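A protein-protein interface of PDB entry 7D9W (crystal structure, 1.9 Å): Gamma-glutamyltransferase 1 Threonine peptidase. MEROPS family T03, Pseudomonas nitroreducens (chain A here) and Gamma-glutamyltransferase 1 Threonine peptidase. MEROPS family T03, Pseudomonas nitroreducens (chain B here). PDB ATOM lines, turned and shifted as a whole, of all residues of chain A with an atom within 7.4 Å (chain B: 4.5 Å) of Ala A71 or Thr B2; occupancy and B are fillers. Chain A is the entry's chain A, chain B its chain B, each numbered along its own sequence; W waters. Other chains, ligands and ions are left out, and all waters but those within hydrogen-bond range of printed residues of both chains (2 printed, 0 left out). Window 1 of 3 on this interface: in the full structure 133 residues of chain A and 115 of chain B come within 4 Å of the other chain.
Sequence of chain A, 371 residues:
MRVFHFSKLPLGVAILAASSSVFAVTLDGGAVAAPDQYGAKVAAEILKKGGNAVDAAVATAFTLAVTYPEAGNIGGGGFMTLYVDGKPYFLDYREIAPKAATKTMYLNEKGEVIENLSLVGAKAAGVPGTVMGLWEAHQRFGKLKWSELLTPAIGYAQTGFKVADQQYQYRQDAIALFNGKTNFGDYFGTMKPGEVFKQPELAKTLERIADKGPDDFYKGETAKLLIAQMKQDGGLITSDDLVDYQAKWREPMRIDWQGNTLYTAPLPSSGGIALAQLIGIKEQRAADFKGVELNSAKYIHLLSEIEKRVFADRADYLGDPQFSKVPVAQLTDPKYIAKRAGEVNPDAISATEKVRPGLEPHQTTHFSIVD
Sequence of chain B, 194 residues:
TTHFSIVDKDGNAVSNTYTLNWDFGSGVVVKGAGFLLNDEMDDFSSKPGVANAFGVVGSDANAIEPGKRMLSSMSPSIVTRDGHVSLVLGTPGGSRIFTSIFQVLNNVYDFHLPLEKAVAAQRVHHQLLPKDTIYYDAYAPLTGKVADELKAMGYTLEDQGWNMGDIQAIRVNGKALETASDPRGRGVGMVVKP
The side-chain amide nitrogen (ND2) of Asn A73 sits at hydrogen-bond distance from the backbone carbonyl oxygen (O) of Thr B19 (3.3 Å). N of Thr B19 sits at hydrogen-bond distance from O of Gly A77. The backbone carbonyl oxygen (O) of Thr B17 is in hydrogen-bond range of the backbone NH (N) of Phe A79 (2.9 Å).
The side-chain carboxylate of Glu A70 lies within hydrogen-bond range of the side-chain amide nitrogen of Gln A167. The backbone carbonyl oxygen (O) of Ala A71 lies within hydrogen-bond range of the side-chain amide nitrogen (ND2) of Asn A73. N of Thr A130 sits at hydrogen-bond distance from O of Gly A76 (3.3 Å). The backbone NH (N) of Gly A77 lies within hydrogen-bond range of the side-chain hydroxyl (OG1) of Thr A130 (3.4 Å). A ring nitrogen (ND1) of His B3 is in hydrogen-bond range of the backbone carbonyl oxygen of Asn B16, 3.1 Å away. The side-chain hydroxyl (OG1) of Thr B17 lies within hydrogen-bond range of a ring nitrogen (ND1) of His B3 (2.6 Å).
Among the printed residues, merely in contact across the chains: Pro A35 with Thr B2 (3.0 Å), Pro A35 with His B3 (3.3 Å), Leu A64 with Tyr B18 (3.2 Å), Ala A65 with Tyr B18 (3.5 Å), Tyr A68 with Thr B2 (3.8 Å), Pro A69 with Leu B20 (3.4 Å), Glu A70 with Leu B20 (3.9 Å), Ala A71 with Thr B1 (3.3 Å), Ala A71 with Thr B2 (3.7 Å), Ala A71 with Thr B19 (3.6 Å), Ala A71 with Leu B20 (3.7 Å), Gly A72 with Thr B2 (3.9 Å), Gly A72 with Tyr B18 (3.3 Å), Asn A73 with Tyr B18 (3.3 Å), Asn A73 with Leu B20 (3.4 Å), Gly A75 with Leu B20 (3.8 Å), Gly A76 with Thr B19 (3.4 Å), Gly A76 with Leu B20 (3.8 Å), Gly A77 with Tyr B18 (3.3 Å), Phe A79 with Asn B16 (3.6 Å) and Thr A130 with Tyr B18 (3.96 Å).
Of the printed residues of chain B, Glu A70 touches Leu B20 (3.9 Å). Ala A71 touches just these residues of chain B: Thr B1, Thr B2, Thr B19 and Leu B20. Of the printed residues of chain B, Phe A79 touches Asn B16 and Thr B17. Printed residues of chain A within 4 Å of Thr B1: Ala A71 (3.3 Å). Of the printed residues of chain A, Thr B2 touches Pro A35, Tyr A68, Ala A71 and Gly A72. Of the printed residues of chain A, Leu B20 touches Pro A69 (3.4 Å), Glu A70 (3.9 Å), Ala A71 (3.7 Å), Asn A73 (3.4 Å), Gly A75 (3.8 Å) and Gly A76 (3.8 Å). Pro B92 touches none of the printed residues of chain A. The nearest printed residue of chain B that does not touch Ala A71 is Tyr B18 (4.2 Å). The nearest printed residue of chain A that does not touch Thr B2 is Leu A64 (4.8 Å).
Hydrophobic or aromatic side chains of chain A within 4 Å of the printed part of chain B: Pro A35, Leu A64, Tyr A68 and Ala A71. Of the 9 printed residues of chain B, 8 touch a printed residue of chain A. Printed residues of chain B that touch a printed residue of chain A: Thr B1, Thr B2, His B3, Asn B16, Thr B17, Tyr B18, Thr B19 and Leu B20. Along chain B the printed residues that touch a printed residue of chain A span positions 1 to 20. Among the printed residues, 24 pairs touch across the chains. Among the printed residues, no Asp or Glu carboxylate lies within 4 Å of a Lys or Arg side-chain nitrogen of the other chain.
Water W1 lies within hydrogen-bond range of the side-chain hydroxyl of Thr B2 (2.8 Å) and the side-chain hydroxyl of Tyr A68 (3.2 Å). Water W2 lies within hydrogen-bond range of O of Glu A70, N of Thr B1, N of Leu B20 and OG1 of Thr B19.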
ATOM      1  N   ALA A  34     -25.400  14.248 -21.559  1.00  0.00           N
ATOM      2  CA  ALA A  34     -24.782  13.048 -22.092  1.00  0.00           C
ATOM      3  C   ALA A  34     -23.667  13.414 -23.057  1.00  0.00           C
ATOM      4  O   ALA A  34     -23.657  14.514 -23.625  1.00  0.00           O
ATOM      5  CB  ALA A  34     -25.814  12.163 -22.805  1.00  0.00           C
ATOM      6  N   PRO A  35     -22.696  12.518 -23.256  1.00  0.00           N
ATOM      7  CA  PRO A  35     -21.540  12.865 -24.093  1.00  0.00           C
ATOM      8  C   PRO A  35     -21.824  12.847 -25.583  1.00  0.00           C
ATOM      9  O   PRO A  35     -20.937  13.223 -26.360  1.00  0.00           O
ATOM     10  CB  PRO A  35     -20.497  11.803 -23.711  1.00  0.00           C
ATOM     11  CG  PRO A  35     -21.302  10.639 -23.242  1.00  0.00           C
ATOM     12  CD  PRO A  35     -22.534  11.211 -22.585  1.00  0.00           C
ATOM     13  N   ASP A  36     -23.011  12.427 -26.014  1.00  0.00           N
ATOM     14  CA  ASP A  36     -23.417  12.640 -27.397  1.00  0.00           C
ATOM     15  C   ASP A  36     -24.932  12.766 -27.478  1.00  0.00           C
ATOM     16  O   ASP A  36     -25.655  12.605 -26.489  1.00  0.00           O
ATOM     17  CB  ASP A  36     -22.858  11.537 -28.321  1.00  0.00           C
ATOM     18  CG  ASP A  36     -23.583  10.200 -28.198  1.00  0.00           C
ATOM     19  OD1 ASP A  36     -24.704  10.128 -27.649  1.00  0.00           O
ATOM     20  OD2 ASP A  36     -23.004   9.195 -28.669  1.00  0.00           O
ATOM     21  N   LEU A  64     -24.632   4.200 -25.412  1.00  0.00           N
ATOM     22  CA  LEU A  64     -23.272   4.671 -25.663  1.00  0.00           C
ATOM     23  C   LEU A  64     -22.296   3.526 -25.938  1.00  0.00           C
ATOM     24  O   LEU A  64     -21.259   3.760 -26.571  1.00  0.00           O
ATOM     25  CB  LEU A  64     -22.786   5.517 -24.480  1.00  0.00           C
ATOM     26  CG  LEU A  64     -23.623   6.771 -24.203  1.00  0.00           C
ATOM     27  CD1 LEU A  64     -23.268   7.370 -22.850  1.00  0.00           C
ATOM     28  CD2 LEU A  64     -23.455   7.814 -25.312  1.00  0.00           C
ATOM     29  N   ALA A  65     -22.595   2.305 -25.475  1.00  0.00           N
ATOM     30  CA  ALA A  65     -21.804   1.144 -25.871  1.00  0.00           C
ATOM     31  C   ALA A  65     -21.897   0.881 -27.370  1.00  0.00           C
ATOM     32  O   ALA A  65     -21.060   0.152 -27.920  1.00  0.00           O
ATOM     33  CB  ALA A  65     -22.254  -0.098 -25.095  1.00  0.00           C
ATOM     34  N   TYR A  68     -20.789   5.335 -28.830  1.00  0.00           N
ATOM     35  CA  TYR A  68     -19.577   5.943 -28.271  1.00  0.00           C
ATOM     36  C   TYR A  68     -18.558   4.852 -27.940  1.00  0.00           C
ATOM     37  O   TYR A  68     -17.973   4.831 -26.857  1.00  0.00           O
ATOM     38  CB  TYR A  68     -19.956   6.759 -27.045  1.00  0.00           C
ATOM     39  CG  TYR A  68     -19.145   8.017 -26.799  1.00  0.00           C
ATOM     40  CD1 TYR A  68     -17.936   7.960 -26.119  1.00  0.00           C
ATOM     41  CD2 TYR A  68     -19.593   9.263 -27.236  1.00  0.00           C
ATOM     42  CE1 TYR A  68     -17.194   9.103 -25.877  1.00  0.00           C
ATOM     43  CE2 TYR A  68     -18.854  10.412 -27.003  1.00  0.00           C
ATOM     44  CZ  TYR A  68     -17.654  10.324 -26.324  1.00  0.00           C
ATOM     45  OH  TYR A  68     -16.913  11.458 -26.086  1.00  0.00           O
ATOM     46  N   PRO A  69     -18.294   3.947 -28.890  1.00  0.00           N
ATOM     47  CA  PRO A  69     -17.470   2.759 -28.601  1.00  0.00           C
ATOM     48  C   PRO A  69     -16.037   3.043 -28.188  1.00  0.00           C
ATOM     49  O   PRO A  69     -15.369   2.109 -27.720  1.00  0.00           O
ATOM     50  CB  PRO A  69     -17.501   1.980 -29.924  1.00  0.00           C
ATOM     51  CG  PRO A  69     -17.724   3.050 -30.968  1.00  0.00           C
ATOM     52  CD  PRO A  69     -18.673   4.020 -30.314  1.00  0.00           C
ATOM     53  N   GLU A  70     -15.526   4.265 -28.355  1.00  0.00           N
ATOM     54  CA  GLU A  70     -14.198   4.554 -27.824  1.00  0.00           C
ATOM     55  C   GLU A  70     -14.173   4.488 -26.298  1.00  0.00           C
ATOM     56  O   GLU A  70     -13.109   4.243 -25.717  1.00  0.00           O
ATOM     57  CB  GLU A  70     -13.709   5.926 -28.303  1.00  0.00           C
ATOM     58  CG  GLU A  70     -14.597   7.123 -27.956  1.00  0.00           C
ATOM     59  CD  GLU A  70     -15.611   7.464 -29.041  1.00  0.00           C
ATOM     60  OE1 GLU A  70     -16.311   6.554 -29.527  1.00  0.00           O
ATOM     61  OE2 GLU A  70     -15.700   8.653 -29.411  1.00  0.00           O
ATOM     62  N   ALA A  71     -15.318   4.678 -25.638  1.00  0.00           N
ATOM     63  CA  ALA A  71     -15.359   4.665 -24.180  1.00  0.00           C
ATOM     64  C   ALA A  71     -16.617   3.991 -23.647  1.00  0.00           C
ATOM     65  O   ALA A  71     -16.539   3.174 -22.724  1.00  0.00           O
ATOM     66  CB  ALA A  71     -15.262   6.095 -23.638  1.00  0.00           C
ATOM     67  N   GLY A  72     -17.780   4.345 -24.188  1.00  0.00           N
ATOM     68  CA  GLY A  72     -18.975   3.573 -23.895  1.00  0.00           C
ATOM     69  C   GLY A  72     -18.752   2.120 -24.270  1.00  0.00           C
ATOM     70  O   GLY A  72     -18.086   1.814 -25.264  1.00  0.00           O
ATOM     71  N   ASN A  73     -19.299   1.210 -23.462  1.00  0.00           N
ATOM     72  CA  ASN A  73     -18.839  -0.167 -23.538  1.00  0.00           C
ATOM     73  C   ASN A  73     -19.766  -1.143 -22.831  1.00  0.00           C
ATOM     74  O   ASN A  73     -20.515  -0.784 -21.922  1.00  0.00           O
ATOM     75  CB  ASN A  73     -17.446  -0.306 -22.906  1.00  0.00           C
ATOM     76  CG  ASN A  73     -17.498  -0.107 -21.388  1.00  0.00           C
ATOM     77  OD1 ASN A  73     -17.688  -1.062 -20.626  1.00  0.00           O
ATOM     78  ND2 ASN A  73     -17.330   1.136 -20.953  1.00  0.00           N
ATOM     79  N   ILE A  74     -19.673  -2.403 -23.261  1.00  0.00           N
ATOM     80  CA  ILE A  74     -19.992  -3.550 -22.413  1.00  0.00           C
ATOM     81  C   ILE A  74     -18.765  -4.402 -22.111  1.00  0.00           C
ATOM     82  O   ILE A  74     -18.865  -5.342 -21.302  1.00  0.00           O
ATOM     83  CB  ILE A  74     -21.108  -4.426 -23.023  1.00  0.00           C
ATOM     84  CG1 ILE A  74     -20.712  -4.943 -24.409  1.00  0.00           C
ATOM     85  CG2 ILE A  74     -22.404  -3.634 -23.080  1.00  0.00           C
ATOM     86  CD1 ILE A  74     -21.714  -5.947 -25.019  1.00  0.00           C
ATOM     87  N   GLY A  75     -17.615  -4.102 -22.716  1.00  0.00           N
ATOM     88  CA  GLY A  75     -16.398  -4.840 -22.443  1.00  0.00           C
ATOM     89  C   GLY A  75     -15.440  -4.165 -21.476  1.00  0.00           C
ATOM     90  O   GLY A  75     -14.274  -4.568 -21.388  1.00  0.00           O
ATOM     91  N   GLY A  76     -15.916  -3.161 -20.731  1.00  0.00           N
ATOM     92  CA  GLY A  76     -15.100  -2.416 -19.787  1.00  0.00           C
ATOM     93  C   GLY A  76     -15.715  -2.399 -18.394  1.00  0.00           C
ATOM     94  O   GLY A  76     -16.247  -3.399 -17.907  1.00  0.00           O
ATOM     95  N   GLY A  77     -15.626  -1.240 -17.745  1.00  0.00           N
ATOM     96  CA  GLY A  77     -16.117  -1.104 -16.386  1.00  0.00           C
ATOM     97  C   GLY A  77     -16.283   0.350 -16.001  1.00  0.00           C
ATOM     98  O   GLY A  77     -16.004   1.262 -16.782  1.00  0.00           O
ATOM     99  N   PHE A  79     -18.120   3.137 -12.620  1.00  0.00           N
ATOM    100  CA  PHE A  79     -18.647   3.454 -11.306  1.00  0.00           C
ATOM    101  C   PHE A  79     -19.924   4.263 -11.491  1.00  0.00           C
ATOM    102  O   PHE A  79     -20.011   5.092 -12.403  1.00  0.00           O
ATOM    103  CB  PHE A  79     -17.704   4.325 -10.465  1.00  0.00           C
ATOM    104  CG  PHE A  79     -16.366   3.725 -10.177  1.00  0.00           C
ATOM    105  CD1 PHE A  79     -16.237   2.477  -9.592  1.00  0.00           C
ATOM    106  CD2 PHE A  79     -15.217   4.454 -10.458  1.00  0.00           C
ATOM    107  CE1 PHE A  79     -14.978   1.961  -9.313  1.00  0.00           C
ATOM    108  CE2 PHE A  79     -13.965   3.944 -10.187  1.00  0.00           C
ATOM    109  CZ  PHE A  79     -13.841   2.698  -9.616  1.00  0.00           C
ATOM    110  N   THR A 130     -19.297  -3.960 -16.743  1.00  0.00           N
ATOM    111  CA  THR A 130     -20.377  -3.027 -17.056  1.00  0.00           C
ATOM    112  C   THR A 130     -21.742  -3.716 -17.101  1.00  0.00           C
ATOM    113  O   THR A 130     -22.725  -3.196 -16.563  1.00  0.00           O
ATOM    114  CB  THR A 130     -20.098  -2.322 -18.383  1.00  0.00           C
ATOM    115  OG1 THR A 130     -18.949  -1.484 -18.244  1.00  0.00           O
ATOM    116  CG2 THR A 130     -21.285  -1.477 -18.807  1.00  0.00           C
ATOM    117  N   GLN A 167     -14.587  11.455 -32.680  1.00  0.00           N
ATOM    118  CA  GLN A 167     -14.608   9.999 -32.663  1.00  0.00           C
ATOM    119  C   GLN A 167     -13.719   9.408 -33.751  1.00  0.00           C
ATOM    120  O   GLN A 167     -12.930   8.492 -33.498  1.00  0.00           O
ATOM    121  CB  GLN A 167     -16.055   9.553 -32.844  1.00  0.00           C
ATOM    122  CG  GLN A 167     -16.314   8.111 -32.663  1.00  0.00           C
ATOM    123  CD  GLN A 167     -17.790   7.835 -32.715  1.00  0.00           C
ATOM    124  OE1 GLN A 167     -18.487   8.301 -33.619  1.00  0.00           O
ATOM    125  NE2 GLN A 167     -18.292   7.116 -31.723  1.00  0.00           N
ATOM    126  N   TYR A 170     -10.018   9.795 -32.927  1.00  0.00           N
ATOM    127  CA  TYR A 170      -9.597   8.763 -31.985  1.00  0.00           C
ATOM    128  C   TYR A 170      -9.423   7.421 -32.691  1.00  0.00           C
ATOM    129  O   TYR A 170      -8.511   6.652 -32.368  1.00  0.00           O
ATOM    130  CB  TYR A 170     -10.614   8.629 -30.851  1.00  0.00           C
ATOM    131  CG  TYR A 170     -10.630   9.765 -29.849  1.00  0.00           C
ATOM    132  CD1 TYR A 170      -9.486  10.509 -29.580  1.00  0.00           C
ATOM    133  CD2 TYR A 170     -11.795  10.086 -29.162  1.00  0.00           C
ATOM    134  CE1 TYR A 170      -9.505  11.543 -28.660  1.00  0.00           C
ATOM    135  CE2 TYR A 170     -11.821  11.118 -28.241  1.00  0.00           C
ATOM    136  CZ  TYR A 170     -10.675  11.842 -27.994  1.00  0.00           C
ATOM    137  N   THR B   1     -12.657   6.781 -21.203  1.00  0.00           N
ATOM    138  CA  THR B   1     -13.703   7.165 -20.262  1.00  0.00           C
ATOM    139  C   THR B   1     -14.725   8.050 -20.980  1.00  0.00           C
ATOM    140  O   THR B   1     -14.398   8.753 -21.934  1.00  0.00           O
ATOM    141  CB  THR B   1     -13.125   7.929 -19.048  1.00  0.00           C
ATOM    142  OG1 THR B   1     -12.025   7.194 -18.490  1.00  0.00           O
ATOM    143  CG2 THR B   1     -14.178   8.138 -17.955  1.00  0.00           C
ATOM    144  N   THR B   2     -15.971   7.982 -20.531  1.00  0.00           N
ATOM    145  CA  THR B   2     -16.951   9.019 -20.811  1.00  0.00           C
ATOM    146  C   THR B   2     -17.858   9.067 -19.589  1.00  0.00           C
ATOM    147  O   THR B   2     -17.813   8.180 -18.731  1.00  0.00           O
ATOM    148  CB  THR B   2     -17.713   8.777 -22.115  1.00  0.00           C
ATOM    149  OG1 THR B   2     -18.565   9.906 -22.366  1.00  0.00           O
ATOM    150  CG2 THR B   2     -18.563   7.511 -22.071  1.00  0.00           C
ATOM    151  N   HIS B   3     -18.650  10.127 -19.482  1.00  0.00           N
ATOM    152  CA  HIS B   3     -19.483  10.320 -18.305  1.00  0.00           C
ATOM    153  C   HIS B   3     -20.846  10.846 -18.728  1.00  0.00           C
ATOM    154  O   HIS B   3     -20.957  11.582 -19.708  1.00  0.00           O
ATOM    155  CB  HIS B   3     -18.840  11.305 -17.317  1.00  0.00           C
ATOM    156  CG  HIS B   3     -19.698  11.584 -16.125  1.00  0.00           C
ATOM    157  ND1 HIS B   3     -19.654  10.814 -14.982  1.00  0.00           N
ATOM    158  CD2 HIS B   3     -20.671  12.502 -15.923  1.00  0.00           C
ATOM    159  CE1 HIS B   3     -20.552  11.257 -14.122  1.00  0.00           C
ATOM    160  NE2 HIS B   3     -21.171  12.290 -14.662  1.00  0.00           N
ATOM    161  N   ASN B  16     -22.704   8.711 -13.785  1.00  0.00           N
ATOM    162  CA  ASN B  16     -22.129   7.452 -14.240  1.00  0.00           C
ATOM    163  C   ASN B  16     -20.909   7.695 -15.112  1.00  0.00           C
ATOM    164  O   ASN B  16     -21.019   8.290 -16.191  1.00  0.00           O
ATOM    165  CB  ASN B  16     -23.155   6.623 -15.013  1.00  0.00           C
ATOM    166  CG  ASN B  16     -22.650   5.242 -15.336  1.00  0.00           C
ATOM    167  OD1 ASN B  16     -22.805   4.323 -14.543  1.00  0.00           O
ATOM    168  ND2 ASN B  16     -21.994   5.096 -16.483  1.00  0.00           N
ATOM    169  N   THR B  17     -19.754   7.221 -14.643  1.00  0.00           N
ATOM    170  CA  THR B  17     -18.490   7.265 -15.370  1.00  0.00           C
ATOM    171  C   THR B  17     -18.077   5.829 -15.682  1.00  0.00           C
ATOM    172  O   THR B  17     -17.984   5.003 -14.771  1.00  0.00           O
ATOM    173  CB  THR B  17     -17.394   7.944 -14.541  1.00  0.00           C
ATOM    174  OG1 THR B  17     -17.879   9.152 -13.946  1.00  0.00           O
ATOM    175  CG2 THR B  17     -16.190   8.275 -15.416  1.00  0.00           C
ATOM    176  N   TYR B  18     -17.828   5.533 -16.955  1.00  0.00           N
ATOM    177  CA  TYR B  18     -17.427   4.184 -17.346  1.00  0.00           C
ATOM    178  C   TYR B  18     -16.507   4.280 -18.551  1.00  0.00           C
ATOM    179  O   TYR B  18     -16.372   5.340 -19.172  1.00  0.00           O
ATOM    180  CB  TYR B  18     -18.676   3.295 -17.539  1.00  0.00           C
ATOM    181  CG  TYR B  18     -19.487   3.376 -18.816  1.00  0.00           C
ATOM    182  CD1 TYR B  18     -19.836   4.592 -19.386  1.00  0.00           C
ATOM    183  CD2 TYR B  18     -19.991   2.215 -19.389  1.00  0.00           C
ATOM    184  CE1 TYR B  18     -20.614   4.636 -20.539  1.00  0.00           C
ATOM    185  CE2 TYR B  18     -20.768   2.250 -20.530  1.00  0.00           C
ATOM    186  CZ  TYR B  18     -21.081   3.463 -21.096  1.00  0.00           C
ATOM    187  OH  TYR B  18     -21.857   3.489 -22.229  1.00  0.00           O
ATOM    188  N   THR B  19     -15.805   3.183 -18.827  1.00  0.00           N
ATOM    189  CA  THR B  19     -14.614   3.298 -19.661  1.00  0.00           C
ATOM    190  C   THR B  19     -14.115   1.946 -20.140  1.00  0.00           C
ATOM    191  O   THR B  19     -14.394   0.905 -19.541  1.00  0.00           O
ATOM    192  CB  THR B  19     -13.494   3.996 -18.863  1.00  0.00           C
ATOM    193  OG1 THR B  19     -12.375   4.282 -19.701  1.00  0.00           O
ATOM    194  CG2 THR B  19     -13.022   3.080 -17.717  1.00  0.00           C
ATOM    195  N   LEU B  20     -13.346   1.995 -21.227  1.00  0.00           N
ATOM    196  CA  LEU B  20     -12.448   0.925 -21.632  1.00  0.00           C
ATOM    197  C   LEU B  20     -11.014   1.173 -21.175  1.00  0.00           C
ATOM    198  O   LEU B  20     -10.145   0.324 -21.403  1.00  0.00           O
ATOM    199  CB  LEU B  20     -12.465   0.775 -23.155  1.00  0.00           C
ATOM    200  CG  LEU B  20     -13.763   0.302 -23.805  1.00  0.00           C
ATOM    201  CD1 LEU B  20     -13.627   0.359 -25.326  1.00  0.00           C
ATOM    202  CD2 LEU B  20     -14.122  -1.096 -23.332  1.00  0.00           C
ATOM    203  N   PRO B  92     -14.420  12.317 -18.144  1.00  0.00           N
ATOM    204  CA  PRO B  92     -13.214  11.541 -18.459  1.00  0.00           C
ATOM    205  C   PRO B  92     -11.969  12.372 -18.161  1.00  0.00           C
ATOM    206  O   PRO B  92     -12.052  13.517 -17.728  1.00  0.00           O
ATOM    207  CB  PRO B  92     -13.366  11.265 -19.956  1.00  0.00           C
ATOM    208  CG  PRO B  92     -14.091  12.480 -20.467  1.00  0.00           C
ATOM    209  CD  PRO B  92     -15.086  12.815 -19.366  1.00  0.00           C
HETATM  210  O   HOH W   1     -16.795  12.019 -22.889  1.00  0.00           O
HETATM  211  O   HOH W   2     -12.211   4.371 -22.914  1.00  0.00           O
